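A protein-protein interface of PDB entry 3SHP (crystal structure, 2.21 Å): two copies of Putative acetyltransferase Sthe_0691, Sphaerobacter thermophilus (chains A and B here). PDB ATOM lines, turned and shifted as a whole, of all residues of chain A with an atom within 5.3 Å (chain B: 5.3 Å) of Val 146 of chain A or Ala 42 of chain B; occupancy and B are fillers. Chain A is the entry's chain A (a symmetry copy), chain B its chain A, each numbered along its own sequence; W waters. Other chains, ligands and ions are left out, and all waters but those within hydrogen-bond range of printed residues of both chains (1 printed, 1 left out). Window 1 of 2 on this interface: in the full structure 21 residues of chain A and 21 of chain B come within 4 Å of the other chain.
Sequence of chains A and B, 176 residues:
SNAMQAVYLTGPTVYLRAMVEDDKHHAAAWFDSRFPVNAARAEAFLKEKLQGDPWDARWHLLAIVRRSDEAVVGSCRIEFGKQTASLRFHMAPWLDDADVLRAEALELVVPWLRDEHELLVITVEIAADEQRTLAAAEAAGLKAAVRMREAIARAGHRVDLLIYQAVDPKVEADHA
O of Glu 43 of chain B sits at hydrogen-bond distance from N of Arg 147 of chain A, 2.9 Å away. The backbone NH (N) of Phe 45 of chain B sits at hydrogen-bond distance from the backbone carbonyl oxygen (O) of Ala 145 of chain A (3.0 Å).
The side-chain carboxylate of Glu 125 of chain B is in salt-bridge range of the guanidinium group of Arg 41 of chain B (2.9 Å). The backbone carbonyl oxygen (O) of Val 146 of chain B is in hydrogen-bond range of the backbone NH (N) of Ile 163 of chain B (3.0 Å). N of Ala 145 of chain A is in hydrogen-bond range of O of Ile 163 of chain A, at 2.8 Å. The backbone NH (N) of Ile 163 of chain A sits at hydrogen-bond distance from the backbone carbonyl oxygen (O) of Val 146 of chain A (3.0 Å). The backbone NH of Met 148 of chain A sits at hydrogen-bond distance from the backbone carbonyl oxygen of Leu 161 of chain A (2.8 Å).
Among the printed residues, pairs that only touch across the chains: Ala 42 of chain A with Val 146 of chain B (3.9 Å), Ala 42 of chain A with Met 148 of chain B (3.9 Å), Glu 43 of chain A with Val 146 of chain B (3.4 Å), Ala 144 of chain A with Phe 45 of chain B (3.7 Å), Ala 145 of chain A with Ala 44 of chain B (3.7 Å), Val 146 of chain A with Ala 42 of chain B (3.9 Å), Val 146 of chain A with Glu 43 of chain B (3.4 Å), Val 146 of chain A with Phe 45 of chain B (3.8 Å), Arg 147 of chain A with Ala 42 of chain B (3.3 Å), Arg 147 of chain A with Phe 45 of chain B (3.4 Å), Met 148 of chain A with Arg 41 of chain B (3.3 Å), Met 148 of chain A with Ala 42 of chain B (3.9 Å), Met 148 of chain A with Met 148 of chain B (3.5 Å) and Leu 162 of chain A with Phe 45 of chain B (3.9 Å).
Of chain B, only Ala 42 (3.9 Å), Glu 43 (3.4 Å) and Phe 45 (3.8 Å) come within 4 Å of Val 146 of chain A. Of the printed residues of chain A, Met 148 of chain B touches Ala 42 (3.9 Å) and Met 148 (3.5 Å). Printed residues of chain B within 4 Å of Glu 43 of chain A: Val 146 (3.4 Å). Printed residues of chain B within 4 Å of Ala 145 of chain A: Ala 44 (3.7 Å) and Phe 45 (3.0 Å). Gln 165 of chain A touches none of the printed residues of chain B. The nearest residue of chain B that does not touch Val 146 of chain A is Val 146 of chain B (4.1 Å). The nearest residue of chain A that does not touch Ala 42 of chain B is Ala 42 of chain A (4.5 Å).
Of the 11 printed residues of chain B, 7 touch a printed residue of chain A. Printed residues of chain B that touch a printed residue of chain A: Arg 41, Ala 42, Glu 43, Ala 44, Phe 45, Val 146 and Met 148. Hydrophobic or aromatic side chains of chain B that line the printed part of chain A: Ala 42, Phe 45, Val 146 and Met 148. Of the 12 printed residues of chain A, 8 touch a printed residue of chain B. Printed residues of chain A that touch a printed residue of chain B: Ala 42, Glu 43, Ala 144, Ala 145, Val 146, Arg 147, Met 148 and Leu 162. Hydrophobic or aromatic side chains of chain A that line the printed part of chain B: Ala 42, Ala 144, Val 146, Met 148 and Leu 162. Among the printed residues, no Asp or Glu carboxylate lies within 4 Å of a Lys or Arg side-chain nitrogen of the other chain.
Ala 42 of chain A touches Val 146 of chain B, and with the chains exchanged Val 146 of chain A touches Ala 42 of chain B. Ala 42 of chain A touches Met 148 of chain B, and with the chains exchanged Met 148 of chain A touches Ala 42 of chain B. Glu 43 of chain A touches Val 146 of chain B, and with the chains exchanged Val 146 of chain A touches Glu 43 of chain B. Met 148 of chain A touches its own counterpart, Met 148 of chain B. Positions printed for both chains: 42, 43, 44, 146, 148 and 163.
Water W1 lies within hydrogen-bond range of the guanidinium group of Arg 147 of chain A, the side-chain carboxylate of Glu 43 of chain B and the backbone carbonyl oxygen of Ala 44 of chain B.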
ATOM      1  N   ALA A  42      28.094   6.051 -12.149  1.00  0.00           N
ATOM      2  CA  ALA A  42      27.542   4.711 -12.097  1.00  0.00           C
ATOM      3  C   ALA A  42      28.616   3.753 -12.533  1.00  0.00           C
ATOM      4  O   ALA A  42      29.593   4.157 -13.170  1.00  0.00           O
ATOM      5  CB  ALA A  42      26.359   4.608 -13.015  1.00  0.00           C
ATOM      6  N   GLU A  43      28.422   2.470 -12.226  1.00  0.00           N
ATOM      7  CA  GLU A  43      29.420   1.455 -12.538  1.00  0.00           C
ATOM      8  C   GLU A  43      28.723   0.101 -12.403  1.00  0.00           C
ATOM      9  O   GLU A  43      27.733  -0.010 -11.673  1.00  0.00           O
ATOM     10  CB  GLU A  43      30.604   1.571 -11.563  1.00  0.00           C
ATOM     11  CG  GLU A  43      30.178   1.423 -10.103  1.00  0.00           C
ATOM     12  CD  GLU A  43      31.209   1.884  -9.093  1.00  0.00           C
ATOM     13  OE1 GLU A  43      31.491   1.076  -8.169  1.00  0.00           O
ATOM     14  OE2 GLU A  43      31.694   3.052  -9.165  1.00  0.00           O
ATOM     15  N   ALA A  44      29.209  -0.919 -13.100  1.00  0.00           N
ATOM     16  CA  ALA A  44      28.698  -2.275 -12.850  1.00  0.00           C
ATOM     17  C   ALA A  44      28.765  -2.574 -11.358  1.00  0.00           C
ATOM     18  O   ALA A  44      29.717  -2.163 -10.682  1.00  0.00           O
ATOM     19  CB  ALA A  44      29.502  -3.321 -13.609  1.00  0.00           C
ATOM     20  N   ALA A 144      31.255  -0.685 -22.992  1.00  0.00           N
ATOM     21  CA  ALA A 144      30.062  -0.045 -22.446  1.00  0.00           C
ATOM     22  C   ALA A 144      29.419  -0.965 -21.432  1.00  0.00           C
ATOM     23  O   ALA A 144      29.077  -2.103 -21.748  1.00  0.00           O
ATOM     24  CB  ALA A 144      29.085   0.290 -23.562  1.00  0.00           C
ATOM     25  N   ALA A 145      29.252  -0.464 -20.216  1.00  0.00           N
ATOM     26  CA  ALA A 145      28.788  -1.293 -19.100  1.00  0.00           C
ATOM     27  C   ALA A 145      27.432  -0.823 -18.572  1.00  0.00           C
ATOM     28  O   ALA A 145      26.597  -1.640 -18.146  1.00  0.00           O
ATOM     29  CB  ALA A 145      29.822  -1.258 -17.979  1.00  0.00           C
ATOM     30  N   VAL A 146      27.219   0.494 -18.599  1.00  0.00           N
ATOM     31  CA  VAL A 146      26.043   1.099 -18.000  1.00  0.00           C
ATOM     32  C   VAL A 146      25.485   2.119 -18.962  1.00  0.00           C
ATOM     33  O   VAL A 146      26.238   2.842 -19.614  1.00  0.00           O
ATOM     34  CB  VAL A 146      26.380   1.798 -16.640  1.00  0.00           C
ATOM     35  CG1 VAL A 146      25.143   2.502 -16.020  1.00  0.00           C
ATOM     36  CG2 VAL A 146      26.961   0.799 -15.647  1.00  0.00           C
ATOM     37  N   ARG A 147      24.160   2.156 -19.059  1.00  0.00           N
ATOM     38  CA  ARG A 147      23.464   3.195 -19.798  1.00  0.00           C
ATOM     39  C   ARG A 147      22.637   4.025 -18.812  1.00  0.00           C
ATOM     40  O   ARG A 147      21.877   3.464 -18.006  1.00  0.00           O
ATOM     41  CB  ARG A 147      22.523   2.576 -20.825  1.00  0.00           C
ATOM     42  CG  ARG A 147      21.816   3.619 -21.677  1.00  0.00           C
ATOM     43  CD  ARG A 147      20.763   2.997 -22.602  1.00  0.00           C
ATOM     44  NE  ARG A 147      21.273   1.948 -23.493  1.00  0.00           N
ATOM     45  CZ  ARG A 147      21.864   2.172 -24.679  1.00  0.00           C
ATOM     46  NH1 ARG A 147      22.061   3.424 -25.134  1.00  0.00           N
ATOM     47  NH2 ARG A 147      22.267   1.135 -25.418  1.00  0.00           N
ATOM     48  N   MET A 148      22.802   5.344 -18.865  1.00  0.00           N
ATOM     49  CA  MET A 148      21.984   6.255 -18.092  1.00  0.00           C
ATOM     50  C   MET A 148      21.156   7.058 -19.085  1.00  0.00           C
ATOM     51  O   MET A 148      21.663   7.998 -19.719  1.00  0.00           O
ATOM     52  CB  MET A 148      22.876   7.163 -17.246  1.00  0.00           C
ATOM     53  CG  MET A 148      23.752   6.382 -16.227  1.00  0.00           C
ATOM     54  SD  MET A 148      24.701   7.568 -15.010  1.00  0.00           S
ATOM     55  CE  MET A 148      23.159   8.463 -14.174  1.00  0.00           C
ATOM     56  N   LEU A 161      24.077   9.137 -20.857  1.00  0.00           N
ATOM     57  CA  LEU A 161      25.438   9.002 -20.365  1.00  0.00           C
ATOM     58  C   LEU A 161      25.777   7.515 -20.343  1.00  0.00           C
ATOM     59  O   LEU A 161      25.007   6.706 -19.801  1.00  0.00           O
ATOM     60  CB  LEU A 161      25.573   9.565 -18.955  1.00  0.00           C
ATOM     61  CG  LEU A 161      27.020   9.538 -18.432  1.00  0.00           C
ATOM     62  CD1 LEU A 161      27.926  10.369 -19.368  1.00  0.00           C
ATOM     63  CD2 LEU A 161      27.131   9.990 -16.941  1.00  0.00           C
ATOM     64  N   LEU A 162      26.924   7.165 -20.910  1.00  0.00           N
ATOM     65  CA  LEU A 162      27.379   5.792 -20.923  1.00  0.00           C
ATOM     66  C   LEU A 162      28.541   5.674 -19.981  1.00  0.00           C
ATOM     67  O   LEU A 162      29.312   6.615 -19.851  1.00  0.00           O
ATOM     68  CB  LEU A 162      27.815   5.383 -22.334  1.00  0.00           C
ATOM     69  CG  LEU A 162      26.761   5.529 -23.442  1.00  0.00           C
ATOM     70  CD1 LEU A 162      27.291   5.046 -24.812  1.00  0.00           C
ATOM     71  CD2 LEU A 162      25.534   4.761 -23.038  1.00  0.00           C
ATOM     72  N   ILE A 163      28.663   4.527 -19.314  1.00  0.00           N
ATOM     73  CA  ILE A 163      29.817   4.241 -18.469  1.00  0.00           C
ATOM     74  C   ILE A 163      30.591   3.090 -19.086  1.00  0.00           C
ATOM     75  O   ILE A 163      30.068   1.970 -19.219  1.00  0.00           O
ATOM     76  CB  ILE A 163      29.416   3.820 -17.047  1.00  0.00           C
ATOM     77  CG1 ILE A 163      28.400   4.795 -16.445  1.00  0.00           C
ATOM     78  CG2 ILE A 163      30.669   3.639 -16.177  1.00  0.00           C
ATOM     79  CD1 ILE A 163      28.973   6.190 -16.134  1.00  0.00           C
ATOM     80  N   GLN A 165      33.930   0.579 -19.051  1.00  0.00           N
ATOM     81  CA  GLN A 165      34.771  -0.081 -18.049  1.00  0.00           C
ATOM     82  C   GLN A 165      35.702  -1.108 -18.650  1.00  0.00           C
ATOM     83  O   GLN A 165      35.401  -1.720 -19.681  1.00  0.00           O
ATOM     84  CB  GLN A 165      33.898  -0.753 -16.981  1.00  0.00           C
ATOM     85  CG  GLN A 165      33.176   0.258 -16.076  1.00  0.00           C
ATOM     86  CD  GLN A 165      32.560  -0.400 -14.838  1.00  0.00           C
ATOM     87  OE1 GLN A 165      31.563  -1.136 -14.933  1.00  0.00           O
ATOM     88  NE2 GLN A 165      33.143  -0.133 -13.677  1.00  0.00           N
ATOM     89  N   ALA B  40      14.002   4.867 -14.080  1.00  0.00           N
ATOM     90  CA  ALA B  40      15.220   4.293 -13.487  1.00  0.00           C
ATOM     91  C   ALA B  40      16.437   4.859 -14.204  1.00  0.00           C
ATOM     92  O   ALA B  40      16.673   4.567 -15.389  1.00  0.00           O
ATOM     93  CB  ALA B  40      15.217   2.762 -13.512  1.00  0.00           C
ATOM     94  N   ARG B  41      17.174   5.670 -13.440  1.00  0.00           N
ATOM     95  CA  ARG B  41      18.362   6.430 -13.794  1.00  0.00           C
ATOM     96  C   ARG B  41      19.521   5.766 -14.558  1.00  0.00           C
ATOM     97  O   ARG B  41      20.229   6.431 -15.323  1.00  0.00           O
ATOM     98  CB  ARG B  41      18.994   6.821 -12.460  1.00  0.00           C
ATOM     99  CG  ARG B  41      19.038   8.197 -12.205  1.00  0.00           C
ATOM    100  CD  ARG B  41      19.434   8.351 -10.759  1.00  0.00           C
ATOM    101  NE  ARG B  41      18.238   8.207  -9.940  1.00  0.00           N
ATOM    102  CZ  ARG B  41      17.977   8.896  -8.828  1.00  0.00           C
ATOM    103  NH1 ARG B  41      16.834   8.656  -8.182  1.00  0.00           N
ATOM    104  NH2 ARG B  41      18.830   9.831  -8.383  1.00  0.00           N
ATOM    105  N   ALA B  42      19.790   4.507 -14.221  1.00  0.00           N
ATOM    106  CA  ALA B  42      20.870   3.753 -14.828  1.00  0.00           C
ATOM    107  C   ALA B  42      20.394   2.339 -15.020  1.00  0.00           C
ATOM    108  O   ALA B  42      19.422   1.916 -14.388  1.00  0.00           O
ATOM    109  CB  ALA B  42      22.075   3.771 -13.932  1.00  0.00           C
ATOM    110  N   GLU B  43      21.100   1.589 -15.866  1.00  0.00           N
ATOM    111  CA  GLU B  43      20.702   0.224 -16.185  1.00  0.00           C
ATOM    112  C   GLU B  43      21.907  -0.438 -16.853  1.00  0.00           C
ATOM    113  O   GLU B  43      22.749   0.259 -17.428  1.00  0.00           O
ATOM    114  CB  GLU B  43      19.484   0.241 -17.124  1.00  0.00           C
ATOM    115  CG  GLU B  43      19.756   1.001 -18.423  1.00  0.00           C
ATOM    116  CD  GLU B  43      18.517   1.367 -19.213  1.00  0.00           C
ATOM    117  OE1 GLU B  43      18.517   1.056 -20.434  1.00  0.00           O
ATOM    118  OE2 GLU B  43      17.575   2.010 -18.661  1.00  0.00           O
ATOM    119  N   ALA B  44      22.011  -1.759 -16.777  1.00  0.00           N
ATOM    120  CA  ALA B  44      23.038  -2.451 -17.569  1.00  0.00           C
ATOM    121  C   ALA B  44      22.936  -2.012 -19.025  1.00  0.00           C
ATOM    122  O   ALA B  44      21.828  -1.805 -19.537  1.00  0.00           O
ATOM    123  CB  ALA B  44      22.878  -3.962 -17.488  1.00  0.00           C
ATOM    124  N   PHE B  45      24.073  -1.852 -19.680  1.00  0.00           N
ATOM    125  CA  PHE B  45      24.076  -1.484 -21.080  1.00  0.00           C
ATOM    126  C   PHE B  45      23.589  -2.658 -21.916  1.00  0.00           C
ATOM    127  O   PHE B  45      24.247  -3.689 -21.975  1.00  0.00           O
ATOM    128  CB  PHE B  45      25.479  -1.095 -21.520  1.00  0.00           C
ATOM    129  CG  PHE B  45      25.571  -0.607 -22.952  1.00  0.00           C
ATOM    130  CD1 PHE B  45      25.465   0.746 -23.245  1.00  0.00           C
ATOM    131  CD2 PHE B  45      25.798  -1.507 -24.005  1.00  0.00           C
ATOM    132  CE1 PHE B  45      25.571   1.211 -24.566  1.00  0.00           C
ATOM    133  CE2 PHE B  45      25.911  -1.057 -25.334  1.00  0.00           C
ATOM    134  CZ  PHE B  45      25.793   0.306 -25.618  1.00  0.00           C
ATOM    135  N   THR B 123      13.601  -3.038 -14.240  1.00  0.00           N
ATOM    136  CA  THR B 123      14.688  -2.225 -13.725  1.00  0.00           C
ATOM    137  C   THR B 123      14.109  -1.381 -12.579  1.00  0.00           C
ATOM    138  O   THR B 123      13.130  -0.633 -12.773  1.00  0.00           O
ATOM    139  CB  THR B 123      15.295  -1.332 -14.859  1.00  0.00           C
ATOM    140  OG1 THR B 123      15.779  -2.160 -15.926  1.00  0.00           O
ATOM    141  CG2 THR B 123      16.458  -0.480 -14.365  1.00  0.00           C
ATOM    142  N   GLU B 125      15.052   1.095  -9.042  1.00  0.00           N
ATOM    143  CA  GLU B 125      15.968   1.888  -8.213  1.00  0.00           C
ATOM    144  C   GLU B 125      15.736   1.543  -6.751  1.00  0.00           C
ATOM    145  O   GLU B 125      14.567   1.564  -6.283  1.00  0.00           O
ATOM    146  CB  GLU B 125      15.703   3.385  -8.394  1.00  0.00           C
ATOM    147  CG  GLU B 125      16.016   3.935  -9.764  1.00  0.00           C
ATOM    148  CD  GLU B 125      16.032   5.492  -9.789  1.00  0.00           C
ATOM    149  OE1 GLU B 125      15.570   6.123  -8.803  1.00  0.00           O
ATOM    150  OE2 GLU B 125      16.500   6.074 -10.802  1.00  0.00           O
ATOM    151  N   VAL B 146      23.797  -2.365 -11.064  1.00  0.00           N
ATOM    152  CA  VAL B 146      24.502  -1.100 -11.168  1.00  0.00           C
ATOM    153  C   VAL B 146      24.657  -0.522  -9.783  1.00  0.00           C
ATOM    154  O   VAL B 146      23.744  -0.609  -8.962  1.00  0.00           O
ATOM    155  CB  VAL B 146      23.732  -0.080 -12.072  1.00  0.00           C
ATOM    156  CG1 VAL B 146      24.444   1.298 -12.141  1.00  0.00           C
ATOM    157  CG2 VAL B 146      23.543  -0.637 -13.478  1.00  0.00           C
ATOM    158  N   MET B 148      25.595   3.180  -8.044  1.00  0.00           N
ATOM    159  CA  MET B 148      25.825   4.602  -8.198  1.00  0.00           C
ATOM    160  C   MET B 148      26.320   5.119  -6.856  1.00  0.00           C
ATOM    161  O   MET B 148      25.527   5.316  -5.921  1.00  0.00           O
ATOM    162  CB  MET B 148      24.529   5.294  -8.621  1.00  0.00           C
ATOM    163  CG  MET B 148      23.979   4.785  -9.982  1.00  0.00           C
ATOM    164  SD  MET B 148      22.465   5.837 -10.606  1.00  0.00           S
ATOM    165  CE  MET B 148      23.338   7.597 -10.739  1.00  0.00           C
ATOM    166  N   ILE B 163      20.807  -0.260  -8.722  1.00  0.00           N
ATOM    167  CA  ILE B 163      19.809  -0.597  -9.733  1.00  0.00           C
ATOM    168  C   ILE B 163      19.706  -2.108  -9.821  1.00  0.00           C
ATOM    169  O   ILE B 163      20.685  -2.794 -10.167  1.00  0.00           O
ATOM    170  CB  ILE B 163      20.185  -0.075 -11.128  1.00  0.00           C
ATOM    171  CG1 ILE B 163      20.583   1.403 -11.080  1.00  0.00           C
ATOM    172  CG2 ILE B 163      19.050  -0.363 -12.123  1.00  0.00           C
ATOM    173  CD1 ILE B 163      19.417   2.359 -10.768  1.00  0.00           C
HETATM  174  O   HOH W   1      20.557  -0.375 -22.095  1.00  0.00           O
